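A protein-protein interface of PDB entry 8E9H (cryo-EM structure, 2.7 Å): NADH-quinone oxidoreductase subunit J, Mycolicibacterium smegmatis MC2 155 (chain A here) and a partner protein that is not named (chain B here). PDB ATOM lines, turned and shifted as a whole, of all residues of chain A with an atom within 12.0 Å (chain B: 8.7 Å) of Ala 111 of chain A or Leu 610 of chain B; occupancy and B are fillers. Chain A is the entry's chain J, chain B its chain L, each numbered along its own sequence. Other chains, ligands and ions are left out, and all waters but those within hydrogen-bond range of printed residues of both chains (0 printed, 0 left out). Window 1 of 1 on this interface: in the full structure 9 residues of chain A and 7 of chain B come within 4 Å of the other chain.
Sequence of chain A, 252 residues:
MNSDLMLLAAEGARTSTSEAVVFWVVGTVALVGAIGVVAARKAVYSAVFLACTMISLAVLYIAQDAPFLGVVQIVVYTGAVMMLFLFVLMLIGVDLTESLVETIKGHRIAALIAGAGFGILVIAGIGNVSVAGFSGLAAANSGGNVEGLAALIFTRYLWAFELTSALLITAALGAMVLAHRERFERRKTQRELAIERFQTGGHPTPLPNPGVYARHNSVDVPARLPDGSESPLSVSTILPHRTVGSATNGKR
OG1 of Thr 103 of chain A is in hydrogen-bond range of NH2 of Arg 606 of chain B, 3.2 Å away.
The side-chain hydroxyl (OG1) of Thr 602 of chain B lies within hydrogen-bond range of the backbone NH (N) of Phe 604 of chain B, 3.2 Å away. The side-chain hydroxyl of Ser 607 of chain B lies within hydrogen-bond range of the side-chain hydroxyl of Thr 602 of chain B (2.7 Å). The backbone carbonyl oxygen (O) of Phe 604 of chain B is in hydrogen-bond range of the side-chain hydroxyl (OG) of Ser 607 of chain B (2.7 Å). The backbone carbonyl oxygen of Ser 607 of chain B sits at hydrogen-bond distance from the side-chain hydroxyl of Ser 611 of chain B (3.2 Å). The side-chain hydroxyl (OG) of Ser 616 of chain B sits at hydrogen-bond distance from the backbone carbonyl oxygen (O) of Leu 613 of chain B, at 3.2 Å.
Among the printed residues, pairs that only touch across the chains: His 107 of chain A with Arg 606 of chain B, Ile 104 of chain A with Arg 606 of chain B, Leu 121 of chain A with Ser 616 of chain B, Ala 114 of chain A with Leu 610 of chain B, Ile 104 of chain A with Phe 604 of chain B, Gly 115 of chain A with Leu 613 of chain B, Ala 110 of chain A with Leu 610 of chain B, Phe 118 of chain A with Ser 616 of chain B, Ala 114 of chain A with Leu 613 of chain B, His 107 of chain A with Ser 607 of chain B, His 107 of chain A with Leu 610 of chain B and Ala 111 of chain A with Leu 610 of chain B.
Of chain B, only Leu 610 comes within 4 Å of Ala 111 of chain A. Leu 610 of chain B touches just these residues of chain A: His 107 (3.9 Å), Ala 110 (3.7 Å), Ala 111 (3.9 Å) and Ala 114 (3.6 Å). Ser 607 of chain B touches just one residue of chain A: His 107. No residue of chain A comes within 4 Å of Ala 609 of chain B. No residue of chain A comes within 4 Å of Ser 611 of chain B. No residue of chain A comes within 4 Å of Met 612 of chain B. Leu 613 of chain B touches just these residues of chain A: Ala 114 and Gly 115. No residue of chain A comes within 4 Å of Gly 614 of chain B. Of the printed residues of chain B, Thr 103 of chain A touches Arg 606 (3.2 Å). Printed residues of chain B within 4 Å of Phe 118 of chain A: Ser 616 (3.8 Å). Printed residues of chain B within 4 Å of His 107 of chain A: Arg 606, Ser 607 and Leu 610. The nearest residue of chain B that does not touch Ala 111 of chain A is Leu 613 of chain B (4.7 Å).
Printed residues of chain B that touch a printed residue of chain A: Phe 604, Arg 606, Ser 607, Leu 610, Leu 613 and Ser 616. Hydrophobic or aromatic side chains of chain B that line the printed part of chain A: Phe 604, Leu 610 and Leu 613. Of the 23 printed residues of chain A, 9 touch a printed residue of chain B. Printed residues of chain A that touch a printed residue of chain B: Thr 103, Ile 104, His 107, Ala 110, Ala 111, Ala 114, Gly 115, Phe 118 and Leu 121. Hydrophobic or aromatic side chains of chain A within 4 Å of the printed part of chain B: Ile 104, His 107, Ala 110, Ala 114, Phe 118 and Leu 121. Among the printed residues, 13 pairs touch across the chains. Among the printed residues, no Asp or Glu carboxylate lies within 4 Å of a Lys or Arg side-chain nitrogen of the other chain.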
ATOM      1  N   VAL A  38      -6.480   7.061 -11.703  1.00  0.00           N
ATOM      2  CA  VAL A  38      -6.386   7.936 -12.866  1.00  0.00           C
ATOM      3  C   VAL A  38      -5.207   8.893 -12.737  1.00  0.00           C
ATOM      4  O   VAL A  38      -4.545   9.215 -13.729  1.00  0.00           O
ATOM      5  CB  VAL A  38      -7.707   8.696 -13.065  1.00  0.00           C
ATOM      6  CG1 VAL A  38      -7.569   9.704 -14.192  1.00  0.00           C
ATOM      7  CG2 VAL A  38      -8.827   7.720 -13.357  1.00  0.00           C
ATOM      8  N   LEU A 100       2.677  12.490 -16.977  1.00  0.00           N
ATOM      9  CA  LEU A 100       1.260  12.793 -17.147  1.00  0.00           C
ATOM     10  C   LEU A 100       1.027  14.107 -17.880  1.00  0.00           C
ATOM     11  O   LEU A 100      -0.080  14.653 -17.824  1.00  0.00           O
ATOM     12  CB  LEU A 100       0.523  12.823 -15.804  1.00  0.00           C
ATOM     13  CG  LEU A 100       0.735  11.621 -14.887  1.00  0.00           C
ATOM     14  CD1 LEU A 100      -0.264  11.654 -13.747  1.00  0.00           C
ATOM     15  CD2 LEU A 100       0.622  10.321 -15.658  1.00  0.00           C
ATOM     16  N   VAL A 101       2.042  14.637 -18.559  1.00  0.00           N
ATOM     17  CA  VAL A 101       1.856  15.840 -19.355  1.00  0.00           C
ATOM     18  C   VAL A 101       1.185  15.473 -20.669  1.00  0.00           C
ATOM     19  O   VAL A 101       1.573  14.507 -21.340  1.00  0.00           O
ATOM     20  CB  VAL A 101       3.205  16.538 -19.594  1.00  0.00           C
ATOM     21  CG1 VAL A 101       3.024  17.736 -20.511  1.00  0.00           C
ATOM     22  CG2 VAL A 101       3.820  16.956 -18.273  1.00  0.00           C
ATOM     23  N   GLU A 102       0.170  16.246 -21.047  1.00  0.00           N
ATOM     24  CA  GLU A 102      -0.582  15.963 -22.263  1.00  0.00           C
ATOM     25  C   GLU A 102       0.343  15.934 -23.471  1.00  0.00           C
ATOM     26  O   GLU A 102       0.904  16.965 -23.855  1.00  0.00           O
ATOM     27  CB  GLU A 102      -1.684  17.003 -22.464  1.00  0.00           C
ATOM     28  N   THR A 103       0.511  14.758 -24.072  1.00  0.00           N
ATOM     29  CA  THR A 103       1.334  14.627 -25.267  1.00  0.00           C
ATOM     30  C   THR A 103       0.556  14.912 -26.540  1.00  0.00           C
ATOM     31  O   THR A 103       1.154  15.304 -27.547  1.00  0.00           O
ATOM     32  CB  THR A 103       1.928  13.222 -25.349  1.00  0.00           C
ATOM     33  OG1 THR A 103       0.908  12.253 -25.080  1.00  0.00           O
ATOM     34  CG2 THR A 103       3.050  13.062 -24.338  1.00  0.00           C
ATOM     35  N   ILE A 104      -0.759  14.722 -26.520  1.00  0.00           N
ATOM     36  CA  ILE A 104      -1.629  15.039 -27.644  1.00  0.00           C
ATOM     37  C   ILE A 104      -2.198  16.427 -27.398  1.00  0.00           C
ATOM     38  O   ILE A 104      -2.856  16.661 -26.377  1.00  0.00           O
ATOM     39  CB  ILE A 104      -2.749  14.001 -27.808  1.00  0.00           C
ATOM     40  CG1 ILE A 104      -2.162  12.599 -27.974  1.00  0.00           C
ATOM     41  CG2 ILE A 104      -3.621  14.347 -29.002  1.00  0.00           C
ATOM     42  CD1 ILE A 104      -3.170  11.494 -27.770  1.00  0.00           C
ATOM     43  N   LYS A 105      -1.948  17.344 -28.327  1.00  0.00           N
ATOM     44  CA  LYS A 105      -2.326  18.735 -28.119  1.00  0.00           C
ATOM     45  C   LYS A 105      -3.817  18.847 -27.835  1.00  0.00           C
ATOM     46  O   LYS A 105      -4.647  18.299 -28.567  1.00  0.00           O
ATOM     47  CB  LYS A 105      -1.958  19.569 -29.344  1.00  0.00           C
ATOM     48  N   GLY A 106      -4.154  19.551 -26.758  1.00  0.00           N
ATOM     49  CA  GLY A 106      -5.535  19.781 -26.397  1.00  0.00           C
ATOM     50  C   GLY A 106      -6.312  18.543 -26.022  1.00  0.00           C
ATOM     51  O   GLY A 106      -7.537  18.621 -25.886  1.00  0.00           O
ATOM     52  N   HIS A 107      -5.648  17.400 -25.849  1.00  0.00           N
ATOM     53  CA  HIS A 107      -6.371  16.173 -25.544  1.00  0.00           C
ATOM     54  C   HIS A 107      -6.803  16.130 -24.087  1.00  0.00           C
ATOM     55  O   HIS A 107      -7.846  15.559 -23.762  1.00  0.00           O
ATOM     56  CB  HIS A 107      -5.514  14.956 -25.871  1.00  0.00           C
ATOM     57  CG  HIS A 107      -6.165  13.656 -25.524  1.00  0.00           C
ATOM     58  ND1 HIS A 107      -7.061  13.027 -26.359  1.00  0.00           N
ATOM     59  CD2 HIS A 107      -6.056  12.869 -24.429  1.00  0.00           C
ATOM     60  CE1 HIS A 107      -7.472  11.905 -25.796  1.00  0.00           C
ATOM     61  NE2 HIS A 107      -6.878  11.786 -24.624  1.00  0.00           N
ATOM     62  N   ARG A 108      -6.007  16.707 -23.189  1.00  0.00           N
ATOM     63  CA  ARG A 108      -6.334  16.629 -21.769  1.00  0.00           C
ATOM     64  C   ARG A 108      -7.633  17.364 -21.468  1.00  0.00           C
ATOM     65  O   ARG A 108      -8.526  16.829 -20.800  1.00  0.00           O
ATOM     66  CB  ARG A 108      -5.187  17.200 -20.942  1.00  0.00           C
ATOM     67  CG  ARG A 108      -5.473  17.274 -19.458  1.00  0.00           C
ATOM     68  CD  ARG A 108      -4.202  17.529 -18.677  1.00  0.00           C
ATOM     69  NE  ARG A 108      -3.403  16.317 -18.552  1.00  0.00           N
ATOM     70  CZ  ARG A 108      -3.639  15.350 -17.677  1.00  0.00           C
ATOM     71  NH1 ARG A 108      -4.646  15.421 -16.822  1.00  0.00           N
ATOM     72  NH2 ARG A 108      -2.847  14.283 -17.662  1.00  0.00           N
ATOM     73  N   ILE A 109      -7.755  18.597 -21.956  1.00  0.00           N
ATOM     74  CA  ILE A 109      -8.958  19.382 -21.699  1.00  0.00           C
ATOM     75  C   ILE A 109     -10.165  18.717 -22.343  1.00  0.00           C
ATOM     76  O   ILE A 109     -11.245  18.639 -21.747  1.00  0.00           O
ATOM     77  CB  ILE A 109      -8.774  20.821 -22.207  1.00  0.00           C
ATOM     78  CG1 ILE A 109      -7.716  21.541 -21.371  1.00  0.00           C
ATOM     79  CG2 ILE A 109     -10.095  21.566 -22.155  1.00  0.00           C
ATOM     80  CD1 ILE A 109      -7.193  22.808 -22.009  1.00  0.00           C
ATOM     81  N   ALA A 110     -10.004  18.241 -23.577  1.00  0.00           N
ATOM     82  CA  ALA A 110     -11.115  17.595 -24.264  1.00  0.00           C
ATOM     83  C   ALA A 110     -11.557  16.341 -23.529  1.00  0.00           C
ATOM     84  O   ALA A 110     -12.756  16.086 -23.389  1.00  0.00           O
ATOM     85  CB  ALA A 110     -10.721  17.263 -25.701  1.00  0.00           C
ATOM     86  N   ALA A 111     -10.603  15.538 -23.058  1.00  0.00           N
ATOM     87  CA  ALA A 111     -10.948  14.326 -22.327  1.00  0.00           C
ATOM     88  C   ALA A 111     -11.648  14.655 -21.019  1.00  0.00           C
ATOM     89  O   ALA A 111     -12.629  14.000 -20.652  1.00  0.00           O
ATOM     90  CB  ALA A 111      -9.693  13.497 -22.066  1.00  0.00           C
ATOM     91  N   LEU A 112     -11.160  15.663 -20.296  1.00  0.00           N
ATOM     92  CA  LEU A 112     -11.824  16.045 -19.057  1.00  0.00           C
ATOM     93  C   LEU A 112     -13.244  16.519 -19.326  1.00  0.00           C
ATOM     94  O   LEU A 112     -14.177  16.146 -18.606  1.00  0.00           O
ATOM     95  CB  LEU A 112     -11.022  17.132 -18.347  1.00  0.00           C
ATOM     96  CG  LEU A 112      -9.722  16.659 -17.698  1.00  0.00           C
ATOM     97  CD1 LEU A 112      -8.857  17.848 -17.330  1.00  0.00           C
ATOM     98  CD2 LEU A 112     -10.005  15.804 -16.479  1.00  0.00           C
ATOM     99  N   ILE A 113     -13.429  17.333 -20.367  1.00  0.00           N
ATOM    100  CA  ILE A 113     -14.761  17.828 -20.700  1.00  0.00           C
ATOM    101  C   ILE A 113     -15.674  16.672 -21.078  1.00  0.00           C
ATOM    102  O   ILE A 113     -16.830  16.607 -20.649  1.00  0.00           O
ATOM    103  CB  ILE A 113     -14.677  18.871 -21.826  1.00  0.00           C
ATOM    104  CG1 ILE A 113     -14.219  20.214 -21.261  1.00  0.00           C
ATOM    105  CG2 ILE A 113     -16.021  19.008 -22.529  1.00  0.00           C
ATOM    106  CD1 ILE A 113     -13.849  21.229 -22.317  1.00  0.00           C
ATOM    107  N   ALA A 114     -15.174  15.750 -21.900  1.00  0.00           N
ATOM    108  CA  ALA A 114     -15.991  14.620 -22.324  1.00  0.00           C
ATOM    109  C   ALA A 114     -16.380  13.753 -21.139  1.00  0.00           C
ATOM    110  O   ALA A 114     -17.535  13.335 -21.020  1.00  0.00           O
ATOM    111  CB  ALA A 114     -15.243  13.793 -23.368  1.00  0.00           C
ATOM    112  N   GLY A 115     -15.431  13.477 -20.244  1.00  0.00           N
ATOM    113  CA  GLY A 115     -15.751  12.681 -19.074  1.00  0.00           C
ATOM    114  C   GLY A 115     -16.770  13.359 -18.183  1.00  0.00           C
ATOM    115  O   GLY A 115     -17.723  12.730 -17.717  1.00  0.00           O
ATOM    116  N   ALA A 116     -16.582  14.655 -17.932  1.00  0.00           N
ATOM    117  CA  ALA A 116     -17.526  15.383 -17.094  1.00  0.00           C
ATOM    118  C   ALA A 116     -18.912  15.383 -17.718  1.00  0.00           C
ATOM    119  O   ALA A 116     -19.913  15.135 -17.037  1.00  0.00           O
ATOM    120  CB  ALA A 116     -17.034  16.811 -16.874  1.00  0.00           C
ATOM    121  N   GLY A 117     -18.991  15.654 -19.020  1.00  0.00           N
ATOM    122  CA  GLY A 117     -20.283  15.672 -19.680  1.00  0.00           C
ATOM    123  C   GLY A 117     -20.957  14.318 -19.655  1.00  0.00           C
ATOM    124  O   GLY A 117     -22.159  14.212 -19.406  1.00  0.00           O
ATOM    125  N   PHE A 118     -20.191  13.258 -19.914  1.00  0.00           N
ATOM    126  CA  PHE A 118     -20.767  11.922 -19.896  1.00  0.00           C
ATOM    127  C   PHE A 118     -21.277  11.568 -18.509  1.00  0.00           C
ATOM    128  O   PHE A 118     -22.375  11.025 -18.362  1.00  0.00           O
ATOM    129  CB  PHE A 118     -19.743  10.893 -20.362  1.00  0.00           C
ATOM    130  CG  PHE A 118     -20.236   9.487 -20.267  1.00  0.00           C
ATOM    131  CD1 PHE A 118     -21.063   8.966 -21.241  1.00  0.00           C
ATOM    132  CD2 PHE A 118     -19.892   8.692 -19.193  1.00  0.00           C
ATOM    133  CE1 PHE A 118     -21.529   7.679 -21.151  1.00  0.00           C
ATOM    134  CE2 PHE A 118     -20.354   7.403 -19.098  1.00  0.00           C
ATOM    135  CZ  PHE A 118     -21.176   6.896 -20.076  1.00  0.00           C
ATOM    136  N   GLY A 119     -20.489  11.859 -17.474  1.00  0.00           N
ATOM    137  CA  GLY A 119     -20.941  11.571 -16.125  1.00  0.00           C
ATOM    138  C   GLY A 119     -22.184  12.356 -15.759  1.00  0.00           C
ATOM    139  O   GLY A 119     -23.122  11.815 -15.168  1.00  0.00           O
ATOM    140  N   ILE A 120     -22.213  13.640 -16.116  1.00  0.00           N
ATOM    141  CA  ILE A 120     -23.373  14.470 -15.817  1.00  0.00           C
ATOM    142  C   ILE A 120     -24.605  13.922 -16.519  1.00  0.00           C
ATOM    143  O   ILE A 120     -25.684  13.819 -15.928  1.00  0.00           O
ATOM    144  CB  ILE A 120     -23.101  15.930 -16.220  1.00  0.00           C
ATOM    145  CG1 ILE A 120     -22.042  16.552 -15.307  1.00  0.00           C
ATOM    146  CG2 ILE A 120     -24.384  16.739 -16.182  1.00  0.00           C
ATOM    147  CD1 ILE A 120     -22.494  16.758 -13.877  1.00  0.00           C
ATOM    148  N   LEU A 121     -24.464  13.565 -17.795  1.00  0.00           N
ATOM    149  CA  LEU A 121     -25.605  13.057 -18.544  1.00  0.00           C
ATOM    150  C   LEU A 121     -26.073  11.722 -17.990  1.00  0.00           C
ATOM    151  O   LEU A 121     -27.278  11.463 -17.913  1.00  0.00           O
ATOM    152  CB  LEU A 121     -25.241  12.930 -20.020  1.00  0.00           C
ATOM    153  CG  LEU A 121     -25.043  14.269 -20.726  1.00  0.00           C
ATOM    154  CD1 LEU A 121     -24.249  14.091 -22.004  1.00  0.00           C
ATOM    155  CD2 LEU A 121     -26.381  14.915 -21.014  1.00  0.00           C
ATOM    156  N   THR B 602      -6.036  10.526 -36.002  1.00  0.00           N
ATOM    157  CA  THR B 602      -4.707  10.884 -35.523  1.00  0.00           C
ATOM    158  C   THR B 602      -3.807   9.673 -35.342  1.00  0.00           C
ATOM    159  O   THR B 602      -2.582   9.820 -35.359  1.00  0.00           O
ATOM    160  CB  THR B 602      -4.801  11.642 -34.199  1.00  0.00           C
ATOM    161  OG1 THR B 602      -5.162  10.735 -33.152  1.00  0.00           O
ATOM    162  CG2 THR B 602      -5.830  12.755 -34.284  1.00  0.00           C
ATOM    163  N   PHE B 604      -3.748   7.890 -32.561  1.00  0.00           N
ATOM    164  CA  PHE B 604      -3.589   7.654 -31.134  1.00  0.00           C
ATOM    165  C   PHE B 604      -4.825   6.949 -30.600  1.00  0.00           C
ATOM    166  O   PHE B 604      -5.948   7.426 -30.789  1.00  0.00           O
ATOM    167  CB  PHE B 604      -3.365   8.970 -30.398  1.00  0.00           C
ATOM    168  CG  PHE B 604      -2.067   9.630 -30.728  1.00  0.00           C
ATOM    169  CD1 PHE B 604      -0.880   9.127 -30.240  1.00  0.00           C
ATOM    170  CD2 PHE B 604      -2.032  10.754 -31.527  1.00  0.00           C
ATOM    171  CE1 PHE B 604       0.317   9.730 -30.541  1.00  0.00           C
ATOM    172  CE2 PHE B 604      -0.837  11.362 -31.833  1.00  0.00           C
ATOM    173  CZ  PHE B 604       0.339  10.849 -31.339  1.00  0.00           C
ATOM    174  N   ALA B 605      -4.620   5.819 -29.924  1.00  0.00           N
ATOM    175  CA  ALA B 605      -5.748   5.091 -29.359  1.00  0.00           C
ATOM    176  C   ALA B 605      -6.542   5.970 -28.406  1.00  0.00           C
ATOM    177  O   ALA B 605      -7.766   5.843 -28.305  1.00  0.00           O
ATOM    178  CB  ALA B 605      -5.253   3.837 -28.642  1.00  0.00           C
ATOM    179  N   ARG B 606      -5.863   6.873 -27.699  1.00  0.00           N
ATOM    180  CA  ARG B 606      -6.556   7.716 -26.734  1.00  0.00           C
ATOM    181  C   ARG B 606      -7.466   8.724 -27.420  1.00  0.00           C
ATOM    182  O   ARG B 606      -8.543   9.036 -26.904  1.00  0.00           O
ATOM    183  CB  ARG B 606      -5.542   8.418 -25.837  1.00  0.00           C
ATOM    184  CG  ARG B 606      -4.840   7.459 -24.900  1.00  0.00           C
ATOM    185  CD  ARG B 606      -4.014   8.161 -23.848  1.00  0.00           C
ATOM    186  NE  ARG B 606      -3.058   9.099 -24.423  1.00  0.00           N
ATOM    187  CZ  ARG B 606      -2.931  10.370 -24.068  1.00  0.00           C
ATOM    188  NH1 ARG B 606      -3.681  10.907 -23.119  1.00  0.00           N
ATOM    189  NH2 ARG B 606      -2.022  11.124 -24.676  1.00  0.00           N
ATOM    190  N   SER B 607      -7.065   9.241 -28.580  1.00  0.00           N
ATOM    191  CA  SER B 607      -7.960  10.117 -29.326  1.00  0.00           C
ATOM    192  C   SER B 607      -9.203   9.372 -29.791  1.00  0.00           C
ATOM    193  O   SER B 607     -10.314   9.912 -29.729  1.00  0.00           O
ATOM    194  CB  SER B 607      -7.223  10.721 -30.516  1.00  0.00           C
ATOM    195  OG  SER B 607      -7.039   9.753 -31.532  1.00  0.00           O
ATOM    196  N   TYR B 608      -9.041   8.134 -30.254  1.00  0.00           N
ATOM    197  CA  TYR B 608     -10.202   7.336 -30.628  1.00  0.00           C
ATOM    198  C   TYR B 608     -11.091   7.079 -29.423  1.00  0.00           C
ATOM    199  O   TYR B 608     -12.321   7.092 -29.535  1.00  0.00           O
ATOM    200  CB  TYR B 608      -9.758   6.013 -31.242  1.00  0.00           C
ATOM    201  CG  TYR B 608      -8.862   6.150 -32.446  1.00  0.00           C
ATOM    202  CD1 TYR B 608      -8.709   7.364 -33.096  1.00  0.00           C
ATOM    203  CD2 TYR B 608      -8.167   5.058 -32.933  1.00  0.00           C
ATOM    204  CE1 TYR B 608      -7.895   7.482 -34.194  1.00  0.00           C
ATOM    205  CE2 TYR B 608      -7.351   5.168 -34.024  1.00  0.00           C
ATOM    206  CZ  TYR B 608      -7.218   6.381 -34.654  1.00  0.00           C
ATOM    207  OH  TYR B 608      -6.400   6.489 -35.752  1.00  0.00           O
ATOM    208  N   ALA B 609     -10.486   6.823 -28.265  1.00  0.00           N
ATOM    209  CA  ALA B 609     -11.272   6.633 -27.054  1.00  0.00           C
ATOM    210  C   ALA B 609     -12.044   7.896 -26.708  1.00  0.00           C
ATOM    211  O   ALA B 609     -13.188   7.828 -26.252  1.00  0.00           O
ATOM    212  CB  ALA B 609     -10.363   6.221 -25.899  1.00  0.00           C
ATOM    213  N   LEU B 610     -11.427   9.060 -26.903  1.00  0.00           N
ATOM    214  CA  LEU B 610     -12.139  10.313 -26.688  1.00  0.00           C
ATOM    215  C   LEU B 610     -13.329  10.428 -27.628  1.00  0.00           C
ATOM    216  O   LEU B 610     -14.432  10.806 -27.214  1.00  0.00           O
ATOM    217  CB  LEU B 610     -11.187  11.490 -26.881  1.00  0.00           C
ATOM    218  CG  LEU B 610     -11.829  12.868 -27.004  1.00  0.00           C
ATOM    219  CD1 LEU B 610     -12.548  13.221 -25.722  1.00  0.00           C
ATOM    220  CD2 LEU B 610     -10.777  13.906 -27.330  1.00  0.00           C
ATOM    221  N   SER B 611     -13.129  10.096 -28.902  1.00  0.00           N
ATOM    222  CA  SER B 611     -14.243  10.143 -29.841  1.00  0.00           C
ATOM    223  C   SER B 611     -15.361   9.211 -29.401  1.00  0.00           C
ATOM    224  O   SER B 611     -16.540   9.582 -29.430  1.00  0.00           O
ATOM    225  CB  SER B 611     -13.767   9.779 -31.246  1.00  0.00           C
ATOM    226  OG  SER B 611     -12.708  10.622 -31.658  1.00  0.00           O
ATOM    227  N   MET B 612     -15.009   7.999 -28.974  1.00  0.00           N
ATOM    228  CA  MET B 612     -16.015   7.059 -28.494  1.00  0.00           C
ATOM    229  C   MET B 612     -16.757   7.601 -27.282  1.00  0.00           C
ATOM    230  O   MET B 612     -17.987   7.528 -27.228  1.00  0.00           O
ATOM    231  CB  MET B 612     -15.362   5.727 -28.144  1.00  0.00           C
ATOM    232  CG  MET B 612     -14.803   4.988 -29.332  1.00  0.00           C
ATOM    233  SD  MET B 612     -13.981   3.480 -28.818  1.00  0.00           S
ATOM    234  CE  MET B 612     -15.393   2.508 -28.319  1.00  0.00           C
ATOM    235  N   LEU B 613     -16.035   8.154 -26.310  1.00  0.00           N
ATOM    236  CA  LEU B 613     -16.672   8.796 -25.172  1.00  0.00           C
ATOM    237  C   LEU B 613     -17.533   9.968 -25.603  1.00  0.00           C
ATOM    238  O   LEU B 613     -18.384  10.416 -24.829  1.00  0.00           O
ATOM    239  CB  LEU B 613     -15.619   9.268 -24.171  1.00  0.00           C
ATOM    240  CG  LEU B 613     -16.154   9.642 -22.790  1.00  0.00           C
ATOM    241  CD1 LEU B 613     -16.754   8.438 -22.106  1.00  0.00           C
ATOM    242  CD2 LEU B 613     -15.053  10.233 -21.941  1.00  0.00           C
ATOM    243  N   GLY B 614     -17.316  10.472 -26.812  1.00  0.00           N
ATOM    244  CA  GLY B 614     -18.288  11.322 -27.468  1.00  0.00           C
ATOM    245  C   GLY B 614     -19.659  10.671 -27.548  1.00  0.00           C
ATOM    246  O   GLY B 614     -20.640  11.330 -27.900  1.00  0.00           O
ATOM    247  N   GLY B 615     -19.743   9.374 -27.232  1.00  0.00           N
ATOM    248  CA  GLY B 615     -21.031   8.725 -27.041  1.00  0.00           C
ATOM    249  C   GLY B 615     -21.899   9.399 -25.998  1.00  0.00           C
ATOM    250  O   GLY B 615     -23.090   9.085 -25.887  1.00  0.00           O
ATOM    251  N   SER B 616     -21.328  10.317 -25.219  1.00  0.00           N
ATOM    252  CA  SER B 616     -22.162  11.224 -24.447  1.00  0.00           C
ATOM    253  C   SER B 616     -23.116  11.973 -25.359  1.00  0.00           C
ATOM    254  O   SER B 616     -24.219  12.339 -24.944  1.00  0.00           O
ATOM    255  CB  SER B 616     -21.292  12.206 -23.668  1.00  0.00           C
ATOM    256  OG  SER B 616     -20.418  12.899 -24.539  1.00  0.00           O
ATOM    257  N   ALA B 617     -22.711  12.207 -26.609  1.00  0.00           N
ATOM    258  CA  ALA B 617     -23.630  12.783 -27.581  1.00  0.00           C
ATOM    259  C   ALA B 617     -24.824  11.867 -27.805  1.00  0.00           C
ATOM    260  O   ALA B 617     -25.969  12.328 -27.842  1.00  0.00           O
ATOM    261  CB  ALA B 617     -22.903  13.052 -28.897  1.00  0.00           C
